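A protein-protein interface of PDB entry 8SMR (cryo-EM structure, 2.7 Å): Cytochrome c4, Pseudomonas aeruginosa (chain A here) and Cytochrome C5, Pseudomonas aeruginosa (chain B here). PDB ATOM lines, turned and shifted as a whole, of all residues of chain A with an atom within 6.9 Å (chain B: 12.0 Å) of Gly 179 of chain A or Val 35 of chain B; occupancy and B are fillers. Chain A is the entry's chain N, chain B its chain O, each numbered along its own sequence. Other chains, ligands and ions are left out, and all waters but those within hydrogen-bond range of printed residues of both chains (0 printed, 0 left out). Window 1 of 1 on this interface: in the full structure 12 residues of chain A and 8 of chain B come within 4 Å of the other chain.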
ATOM      1  N   VAL A  83     -13.300  -6.527   9.368  1.00  0.00           N
ATOM      2  CA  VAL A  83     -12.397  -7.659   9.194  1.00  0.00           C
ATOM      3  C   VAL A  83     -12.101  -7.820   7.711  1.00  0.00           C
ATOM      4  O   VAL A  83     -13.025  -7.907   6.892  1.00  0.00           O
ATOM      5  CB  VAL A  83     -12.994  -8.952   9.776  1.00  0.00           C
ATOM      6  CG1 VAL A  83     -11.994 -10.094   9.669  1.00  0.00           C
ATOM      7  CG2 VAL A  83     -13.417  -8.738  11.221  1.00  0.00           C
ATOM      8  N   GLY A  84     -10.818  -7.858   7.368  1.00  0.00           N
ATOM      9  CA  GLY A  84     -10.391  -8.114   6.011  1.00  0.00           C
ATOM     10  C   GLY A  84     -10.229  -9.598   5.755  1.00  0.00           C
ATOM     11  O   GLY A  84     -10.785 -10.445   6.458  1.00  0.00           O
ATOM     12  N   MET A  85      -9.447  -9.914   4.727  1.00  0.00           N
ATOM     13  CA  MET A  85      -9.185 -11.289   4.332  1.00  0.00           C
ATOM     14  C   MET A  85      -7.688 -11.556   4.367  1.00  0.00           C
ATOM     15  O   MET A  85      -6.883 -10.677   4.044  1.00  0.00           O
ATOM     16  CB  MET A  85      -9.729 -11.579   2.929  1.00  0.00           C
ATOM     17  CG  MET A  85     -11.080 -10.946   2.634  1.00  0.00           C
ATOM     18  SD  MET A  85     -12.236 -12.076   1.835  1.00  0.00           S
ATOM     19  CE  MET A  85     -12.495 -13.284   3.132  1.00  0.00           C
ATOM     20  N   ALA A  86      -7.323 -12.770   4.764  1.00  0.00           N
ATOM     21  CA  ALA A  86      -5.934 -13.195   4.775  1.00  0.00           C
ATOM     22  C   ALA A  86      -5.570 -13.846   3.446  1.00  0.00           C
ATOM     23  O   ALA A  86      -6.404 -14.477   2.790  1.00  0.00           O
ATOM     24  CB  ALA A  86      -5.679 -14.174   5.922  1.00  0.00           C
ATOM     25  N   ASP A  87      -4.316 -13.684   3.055  1.00  0.00           N
ATOM     26  CA  ASP A  87      -3.832 -14.304   1.829  1.00  0.00           C
ATOM     27  C   ASP A  87      -3.764 -15.817   2.021  1.00  0.00           C
ATOM     28  O   ASP A  87      -3.124 -16.284   2.969  1.00  0.00           O
ATOM     29  CB  ASP A  87      -2.459 -13.746   1.464  1.00  0.00           C
ATOM     30  CG  ASP A  87      -1.909 -14.326   0.175  1.00  0.00           C
ATOM     31  OD1 ASP A  87      -2.651 -15.043  -0.526  1.00  0.00           O
ATOM     32  OD2 ASP A  87      -0.730 -14.062  -0.139  1.00  0.00           O
ATOM     33  N   VAL A  91      -1.754 -17.566   5.106  1.00  0.00           N
ATOM     34  CA  VAL A  91      -2.567 -17.688   6.310  1.00  0.00           C
ATOM     35  C   VAL A  91      -2.020 -18.772   7.230  1.00  0.00           C
ATOM     36  O   VAL A  91      -2.087 -18.648   8.456  1.00  0.00           O
ATOM     37  CB  VAL A  91      -4.038 -17.947   5.939  1.00  0.00           C
ATOM     38  CG1 VAL A  91      -4.237 -19.385   5.488  1.00  0.00           C
ATOM     39  CG2 VAL A  91      -4.940 -17.619   7.118  1.00  0.00           C
ATOM     40  N   GLU A  95      -0.880 -17.730  10.872  1.00  0.00           N
ATOM     41  CA  GLU A  95      -1.633 -18.320  11.971  1.00  0.00           C
ATOM     42  C   GLU A  95      -0.710 -19.052  12.932  1.00  0.00           C
ATOM     43  O   GLU A  95      -0.849 -18.931  14.154  1.00  0.00           O
ATOM     44  CB  GLU A  95      -2.691 -19.274  11.417  1.00  0.00           C
ATOM     45  CG  GLU A  95      -3.479 -20.016  12.478  1.00  0.00           C
ATOM     46  CD  GLU A  95      -4.600 -20.848  11.890  1.00  0.00           C
ATOM     47  OE1 GLU A  95      -4.305 -21.883  11.260  1.00  0.00           O
ATOM     48  OE2 GLU A  95      -5.777 -20.464  12.056  1.00  0.00           O
ATOM     49  N   GLY A 130      -6.961  -7.882  15.413  1.00  0.00           N
ATOM     50  CA  GLY A 130      -7.754  -8.582  14.423  1.00  0.00           C
ATOM     51  C   GLY A 130      -8.530  -7.658  13.510  1.00  0.00           C
ATOM     52  O   GLY A 130      -9.260  -6.778  13.976  1.00  0.00           O
ATOM     53  N   GLY A 131      -8.376  -7.851  12.202  1.00  0.00           N
ATOM     54  CA  GLY A 131      -9.039  -7.029  11.217  1.00  0.00           C
ATOM     55  C   GLY A 131      -8.275  -5.791  10.807  1.00  0.00           C
ATOM     56  O   GLY A 131      -8.684  -5.118   9.853  1.00  0.00           O
ATOM     57  N   GLN A 132      -7.180  -5.468  11.492  1.00  0.00           N
ATOM     58  CA  GLN A 132      -6.371  -4.323  11.106  1.00  0.00           C
ATOM     59  C   GLN A 132      -5.737  -4.569   9.743  1.00  0.00           C
ATOM     60  O   GLN A 132      -5.451  -5.707   9.362  1.00  0.00           O
ATOM     61  CB  GLN A 132      -5.290  -4.057  12.155  1.00  0.00           C
ATOM     62  CG  GLN A 132      -4.495  -2.778  11.933  1.00  0.00           C
ATOM     63  CD  GLN A 132      -5.366  -1.538  11.952  1.00  0.00           C
ATOM     64  OE1 GLN A 132      -5.887  -1.117  10.921  1.00  0.00           O
ATOM     65  NE2 GLN A 132      -5.529  -0.946  13.129  1.00  0.00           N
ATOM     66  N   ALA A 134      -3.435  -5.291   6.816  1.00  0.00           N
ATOM     67  CA  ALA A 134      -2.197  -6.060   6.799  1.00  0.00           C
ATOM     68  C   ALA A 134      -0.999  -5.159   6.540  1.00  0.00           C
ATOM     69  O   ALA A 134       0.065  -5.343   7.141  1.00  0.00           O
ATOM     70  CB  ALA A 134      -2.278  -7.163   5.746  1.00  0.00           C
ATOM     71  N   ILE A 173       2.141 -12.943   9.181  1.00  0.00           N
ATOM     72  CA  ILE A 173       1.387 -12.631  10.387  1.00  0.00           C
ATOM     73  C   ILE A 173       0.481 -11.431  10.152  1.00  0.00           C
ATOM     74  O   ILE A 173      -0.633 -11.372  10.675  1.00  0.00           O
ATOM     75  CB  ILE A 173       2.346 -12.414  11.573  1.00  0.00           C
ATOM     76  CG1 ILE A 173       1.706 -12.916  12.869  1.00  0.00           C
ATOM     77  CG2 ILE A 173       2.740 -10.951  11.712  1.00  0.00           C
ATOM     78  CD1 ILE A 173       2.698 -13.149  13.977  1.00  0.00           C
ATOM     79  N   SER A 174       0.934 -10.457   9.357  1.00  0.00           N
ATOM     80  CA  SER A 174       0.084  -9.318   9.033  1.00  0.00           C
ATOM     81  C   SER A 174      -1.130  -9.754   8.224  1.00  0.00           C
ATOM     82  O   SER A 174      -2.248  -9.294   8.479  1.00  0.00           O
ATOM     83  CB  SER A 174       0.885  -8.268   8.266  1.00  0.00           C
ATOM     84  OG  SER A 174       2.078  -7.936   8.952  1.00  0.00           O
ATOM     85  N   SER A 175      -0.931 -10.641   7.248  1.00  0.00           N
ATOM     86  CA  SER A 175      -2.063 -11.144   6.477  1.00  0.00           C
ATOM     87  C   SER A 175      -3.050 -11.877   7.377  1.00  0.00           C
ATOM     88  O   SER A 175      -4.267 -11.654   7.307  1.00  0.00           O
ATOM     89  CB  SER A 175      -1.565 -12.060   5.359  1.00  0.00           C
ATOM     90  OG  SER A 175      -2.449 -12.040   4.254  1.00  0.00           O
ATOM     91  N   TYR A 176      -2.537 -12.749   8.250  1.00  0.00           N
ATOM     92  CA  TYR A 176      -3.413 -13.481   9.159  1.00  0.00           C
ATOM     93  C   TYR A 176      -4.170 -12.531  10.079  1.00  0.00           C
ATOM     94  O   TYR A 176      -5.372 -12.704  10.309  1.00  0.00           O
ATOM     95  CB  TYR A 176      -2.598 -14.482   9.975  1.00  0.00           C
ATOM     96  CG  TYR A 176      -3.386 -15.146  11.080  1.00  0.00           C
ATOM     97  CD1 TYR A 176      -4.246 -16.198  10.807  1.00  0.00           C
ATOM     98  CD2 TYR A 176      -3.269 -14.721  12.395  1.00  0.00           C
ATOM     99  CE1 TYR A 176      -4.969 -16.807  11.810  1.00  0.00           C
ATOM    100  CE2 TYR A 176      -3.988 -15.325  13.406  1.00  0.00           C
ATOM    101  CZ  TYR A 176      -4.836 -16.368  13.108  1.00  0.00           C
ATOM    102  OH  TYR A 176      -5.555 -16.974  14.112  1.00  0.00           O
ATOM    103  N   ILE A 177      -3.484 -11.519  10.612  1.00  0.00           N
ATOM    104  CA  ILE A 177      -4.132 -10.547  11.485  1.00  0.00           C
ATOM    105  C   ILE A 177      -5.229  -9.812  10.731  1.00  0.00           C
ATOM    106  O   ILE A 177      -6.315  -9.563  11.269  1.00  0.00           O
ATOM    107  CB  ILE A 177      -3.084  -9.575  12.060  1.00  0.00           C
ATOM    108  CG1 ILE A 177      -2.279 -10.259  13.164  1.00  0.00           C
ATOM    109  CG2 ILE A 177      -3.754  -8.319  12.598  1.00  0.00           C
ATOM    110  CD1 ILE A 177      -0.951  -9.597  13.453  1.00  0.00           C
ATOM    111  N   GLN A 178      -4.965  -9.452   9.474  1.00  0.00           N
ATOM    112  CA  GLN A 178      -5.992  -8.803   8.670  1.00  0.00           C
ATOM    113  C   GLN A 178      -7.211  -9.700   8.525  1.00  0.00           C
ATOM    114  O   GLN A 178      -8.351  -9.235   8.630  1.00  0.00           O
ATOM    115  CB  GLN A 178      -5.431  -8.435   7.298  1.00  0.00           C
ATOM    116  CG  GLN A 178      -6.458  -7.837   6.355  1.00  0.00           C
ATOM    117  CD  GLN A 178      -5.826  -7.157   5.161  1.00  0.00           C
ATOM    118  OE1 GLN A 178      -5.529  -5.965   5.197  1.00  0.00           O
ATOM    119  NE2 GLN A 178      -5.620  -7.915   4.090  1.00  0.00           N
ATOM    120  N   GLY A 179      -6.992 -10.994   8.289  1.00  0.00           N
ATOM    121  CA  GLY A 179      -8.108 -11.920   8.218  1.00  0.00           C
ATOM    122  C   GLY A 179      -8.675 -12.349   9.555  1.00  0.00           C
ATOM    123  O   GLY A 179      -9.761 -12.933   9.591  1.00  0.00           O
ATOM    124  N   LEU A 180      -7.974 -12.068  10.650  1.00  0.00           N
ATOM    125  CA  LEU A 180      -8.353 -12.581  11.959  1.00  0.00           C
ATOM    126  C   LEU A 180      -9.583 -11.865  12.502  1.00  0.00           C
ATOM    127  O   LEU A 180      -9.799 -10.679  12.239  1.00  0.00           O
ATOM    128  CB  LEU A 180      -7.189 -12.427  12.939  1.00  0.00           C
ATOM    129  CG  LEU A 180      -7.421 -12.882  14.380  1.00  0.00           C
ATOM    130  CD1 LEU A 180      -7.699 -14.373  14.437  1.00  0.00           C
ATOM    131  CD2 LEU A 180      -6.222 -12.529  15.240  1.00  0.00           C
ATOM    132  N   HIS A 181     -10.389 -12.598  13.265  1.00  0.00           N
ATOM    133  CA  HIS A 181     -11.535 -12.021  13.960  1.00  0.00           C
ATOM    134  C   HIS A 181     -11.992 -12.943  15.086  1.00  0.00           C
ATOM    135  O   HIS A 181     -11.716 -14.142  15.076  1.00  0.00           O
ATOM    136  CB  HIS A 181     -12.690 -11.765  12.992  1.00  0.00           C
ATOM    137  CG  HIS A 181     -13.268 -13.009  12.394  1.00  0.00           C
ATOM    138  ND1 HIS A 181     -12.693 -13.658  11.324  1.00  0.00           N
ATOM    139  CD2 HIS A 181     -14.375 -13.720  12.715  1.00  0.00           C
ATOM    140  CE1 HIS A 181     -13.418 -14.718  11.013  1.00  0.00           C
ATOM    141  NE2 HIS A 181     -14.444 -14.778  11.842  1.00  0.00           N
ATOM    142  OXT HIS A 181     -12.649 -12.511  16.033  1.00  0.00           O
ATOM    143  N   GLU B  30     -12.574 -26.419  19.158  1.00  0.00           N
ATOM    144  CA  GLU B  30     -12.357 -25.481  18.064  1.00  0.00           C
ATOM    145  C   GLU B  30     -11.528 -24.291  18.547  1.00  0.00           C
ATOM    146  O   GLU B  30     -11.837 -23.716  19.600  1.00  0.00           O
ATOM    147  CB  GLU B  30     -13.694 -24.997  17.508  1.00  0.00           C
ATOM    148  CG  GLU B  30     -13.604 -24.403  16.114  1.00  0.00           C
ATOM    149  CD  GLU B  30     -13.467 -25.464  15.038  1.00  0.00           C
ATOM    150  OE1 GLU B  30     -14.507 -25.951  14.547  1.00  0.00           O
ATOM    151  OE2 GLU B  30     -12.320 -25.807  14.683  1.00  0.00           O
ATOM    152  N   PRO B  31     -10.481 -23.890  17.821  1.00  0.00           N
ATOM    153  CA  PRO B  31      -9.697 -22.728  18.255  1.00  0.00           C
ATOM    154  C   PRO B  31     -10.541 -21.463  18.287  1.00  0.00           C
ATOM    155  O   PRO B  31     -11.457 -21.277  17.483  1.00  0.00           O
ATOM    156  CB  PRO B  31      -8.584 -22.633  17.204  1.00  0.00           C
ATOM    157  CG  PRO B  31      -8.504 -23.987  16.603  1.00  0.00           C
ATOM    158  CD  PRO B  31      -9.902 -24.514  16.619  1.00  0.00           C
ATOM    159  N   VAL B  32     -10.220 -20.587  19.239  1.00  0.00           N
ATOM    160  CA  VAL B  32     -10.970 -19.345  19.390  1.00  0.00           C
ATOM    161  C   VAL B  32     -10.769 -18.444  18.178  1.00  0.00           C
ATOM    162  O   VAL B  32     -11.728 -17.874  17.646  1.00  0.00           O
ATOM    163  CB  VAL B  32     -10.562 -18.638  20.694  1.00  0.00           C
ATOM    164  CG1 VAL B  32     -11.106 -17.214  20.727  1.00  0.00           C
ATOM    165  CG2 VAL B  32     -11.045 -19.433  21.894  1.00  0.00           C
ATOM    166  N   GLY B  33      -9.527 -18.301  17.722  1.00  0.00           N
ATOM    167  CA  GLY B  33      -9.222 -17.391  16.637  1.00  0.00           C
ATOM    168  C   GLY B  33      -9.707 -17.869  15.286  1.00  0.00           C
ATOM    169  O   GLY B  33      -9.241 -18.892  14.776  1.00  0.00           O
ATOM    170  N   LYS B  34     -10.645 -17.135  14.695  1.00  0.00           N
ATOM    171  CA  LYS B  34     -11.146 -17.419  13.359  1.00  0.00           C
ATOM    172  C   LYS B  34     -10.586 -16.396  12.380  1.00  0.00           C
ATOM    173  O   LYS B  34     -10.546 -15.198  12.674  1.00  0.00           O
ATOM    174  CB  LYS B  34     -12.676 -17.392  13.328  1.00  0.00           C
ATOM    175  CG  LYS B  34     -13.328 -18.747  13.560  1.00  0.00           C
ATOM    176  CD  LYS B  34     -14.207 -18.741  14.800  1.00  0.00           C
ATOM    177  CE  LYS B  34     -15.498 -17.972  14.566  1.00  0.00           C
ATOM    178  NZ  LYS B  34     -16.220 -17.691  15.837  1.00  0.00           N
ATOM    179  N   VAL B  35     -10.154 -16.875  11.216  1.00  0.00           N
ATOM    180  CA  VAL B  35      -9.477 -16.051  10.220  1.00  0.00           C
ATOM    181  C   VAL B  35     -10.259 -16.117   8.917  1.00  0.00           C
ATOM    182  O   VAL B  35     -10.592 -17.208   8.440  1.00  0.00           O
ATOM    183  CB  VAL B  35      -8.020 -16.503  10.009  1.00  0.00           C
ATOM    184  CG1 VAL B  35      -7.964 -17.934   9.490  1.00  0.00           C
ATOM    185  CG2 VAL B  35      -7.295 -15.559   9.057  1.00  0.00           C
ATOM    186  N   CYS B  36     -10.556 -14.951   8.349  1.00  0.00           N
ATOM    187  CA  CYS B  36     -11.146 -14.859   7.022  1.00  0.00           C
ATOM    188  C   CYS B  36     -10.041 -14.944   5.980  1.00  0.00           C
ATOM    189  O   CYS B  36      -8.997 -14.298   6.119  1.00  0.00           O
ATOM    190  CB  CYS B  36     -11.925 -13.552   6.862  1.00  0.00           C
ATOM    191  SG  CYS B  36     -13.315 -13.364   7.999  1.00  0.00           S
ATOM    192  N   VAL B  37     -10.271 -15.740   4.939  1.00  0.00           N
ATOM    193  CA  VAL B  37      -9.284 -15.964   3.892  1.00  0.00           C
ATOM    194  C   VAL B  37      -9.935 -15.713   2.541  1.00  0.00           C
ATOM    195  O   VAL B  37     -11.111 -16.023   2.329  1.00  0.00           O
ATOM    196  CB  VAL B  37      -8.696 -17.391   3.958  1.00  0.00           C
ATOM    197  CG1 VAL B  37      -7.708 -17.615   2.827  1.00  0.00           C
ATOM    198  CG2 VAL B  37      -8.031 -17.627   5.304  1.00  0.00           C
ATOM    199  N   GLN B  38      -9.158 -15.139   1.623  1.00  0.00           N
ATOM    200  CA  GLN B  38      -9.665 -14.854   0.288  1.00  0.00           C
ATOM    201  C   GLN B  38     -10.138 -16.138  -0.381  1.00  0.00           C
ATOM    202  O   GLN B  38      -9.444 -17.158  -0.358  1.00  0.00           O
ATOM    203  CB  GLN B  38      -8.579 -14.187  -0.556  1.00  0.00           C
ATOM    204  CG  GLN B  38      -8.117 -12.840  -0.025  1.00  0.00           C
ATOM    205  CD  GLN B  38      -6.884 -12.324  -0.741  1.00  0.00           C
ATOM    206  OE1 GLN B  38      -6.321 -13.003  -1.599  1.00  0.00           O
ATOM    207  NE2 GLN B  38      -6.456 -11.118  -0.387  1.00  0.00           N
ATOM    208  N   GLY B  39     -11.322 -16.083  -0.980  1.00  0.00           N
ATOM    209  CA  GLY B  39     -11.896 -17.241  -1.639  1.00  0.00           C
ATOM    210  C   GLY B  39     -12.146 -18.391  -0.684  1.00  0.00           C
ATOM    211  O   GLY B  39     -12.252 -18.195   0.526  1.00  0.00           O
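The backbone NH of Ala 86 of chain A lies within hydrogen-bond range of the backbone carbonyl oxygen of Cys 36 of chain B (2.6 Å).
The backbone NH of Gln 38 of chain B is in hydrogen-bond range of the backbone carbonyl oxygen of Ala 86 of chain A (3.1 Å).
The backbone carbonyl oxygen (O) of Gly 179 of chain A is in hydrogen-bond range of the backbone NH (N) of Cys 36 of chain B.
The backbone carbonyl oxygen of Lys 34 of chain B is in hydrogen-bond range of the backbone NH of His 181 of chain A (2.7 Å).
ND1 of His 181 of chain A sits close to SG of Cys 36 of chain B (3.4 Å).
The backbone NH of Gly 84 of chain A sits at hydrogen-bond distance from the backbone carbonyl oxygen of Gln 178 of chain A, at 3.1 Å.
O of Met 85 of chain A is in hydrogen-bond range of NE2 of Gln 178 of chain A, at 3.0 Å.
The backbone carbonyl oxygen of Leu 180 of chain A lies within hydrogen-bond range of the backbone NH of Gly 131 of chain A, 3.2 Å away.
ND1 of His 181 of chain A is in hydrogen-bond range of O of Gly 179 of chain A (3.5 Å).
Val 83 of chain A touches Cys 36 of chain B (CG1 to SG, 3.9 Å).
Gly 84 of chain A touches Cys 36 of chain B.
CE of Met 85 of chain A touches O of Val 37 of chain B (3.2 Å).
Met 85 of chain A touches Gln 38 of chain B (CB to CG, 3.6 Å).
CG2 of Val 35 of chain B touches CB of Ala 86 of chain A (3.8 Å).
Val 91 of chain A touches Val 37 of chain B.
O of Gly 179 of chain A touches O of Lys 34 of chain B, 3.9 Å away.
Gly 179 of chain A touches Val 35 of chain B (O to CA, 3.2 Å).
Leu 180 of chain A touches Lys 34 of chain B.
N of Leu 180 of chain A touches CG2 of Val 35 of chain B, at 3.9 Å.
Val 83 of chain A touches just one residue of chain B: Cys 36.
Gly 84 of chain A touches one residue of chain B.
Ala 86 of chain A touches just these residues of chain B: Val 35, Cys 36, Val 37 and Gln 38.
Val 91 of chain A touches just these residues of chain B: Val 35 (3.7 Å) and Val 37 (3.6 Å).
No residue of chain B comes within 4 Å of Gly 130 of chain A.
No residue of chain B comes within 4 Å of Ser 175 of chain A.
Of chain B, only Val 35 comes within 4 Å of Tyr 176 of chain A.
No residue of chain B comes within 4 Å of Gln 178 of chain A.
Of chain B, only Lys 34, Val 35 and Cys 36 come within 4 Å of His 181 of chain A.
Of the printed residues of chain A, Lys 34 of chain B touches Gly 179 (3.9 Å), Leu 180 (3.4 Å) and His 181 (2.7 Å).
Printed residues of chain A within 4 Å of Cys 36 of chain B: Val 83, Gly 84, Met 85, Ala 86, Gly 179 and His 181.
Of the printed residues of chain A, Val 37 of chain B touches Met 85 (3.2 Å), Ala 86 (3.4 Å) and Val 91 (3.6 Å).
The nearest residue of chain B that does not touch Gly 179 of chain A is Val 37 of chain B (5.5 Å).
The nearest residue of chain A that does not touch Val 35 of chain B is Glu 95 of chain A (4.2 Å).
The nearest printed residue of chain A that does not touch Gln 38 of chain B is Asp 87 of chain A (4.3 Å).
Of the 20 printed residues of chain A, 9 touch a printed residue of chain B.
Printed residues of chain A that touch a printed residue of chain B: Val 83, Gly 84, Met 85, Ala 86, Val 91, Tyr 176, Gly 179, Leu 180 and His 181.
Hydrophobic or aromatic side chains of chain A within 4 Å of the printed part of chain B: Val 83, Met 85, Ala 86, Val 91, Tyr 176, Leu 180 and His 181.
Of the 10 printed residues of chain B, 5 touch a printed residue of chain A.
Hydrophobic or aromatic side chains of chain B within 4 Å of the printed part of chain A: Val 35 and Val 37.
Along chain B the printed residues that touch a printed residue of chain A span positions 34 to 38.
Among the printed residues, no Asp or Glu carboxylate lies within 4 Å of a Lys or Arg side-chain nitrogen of the other chain.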
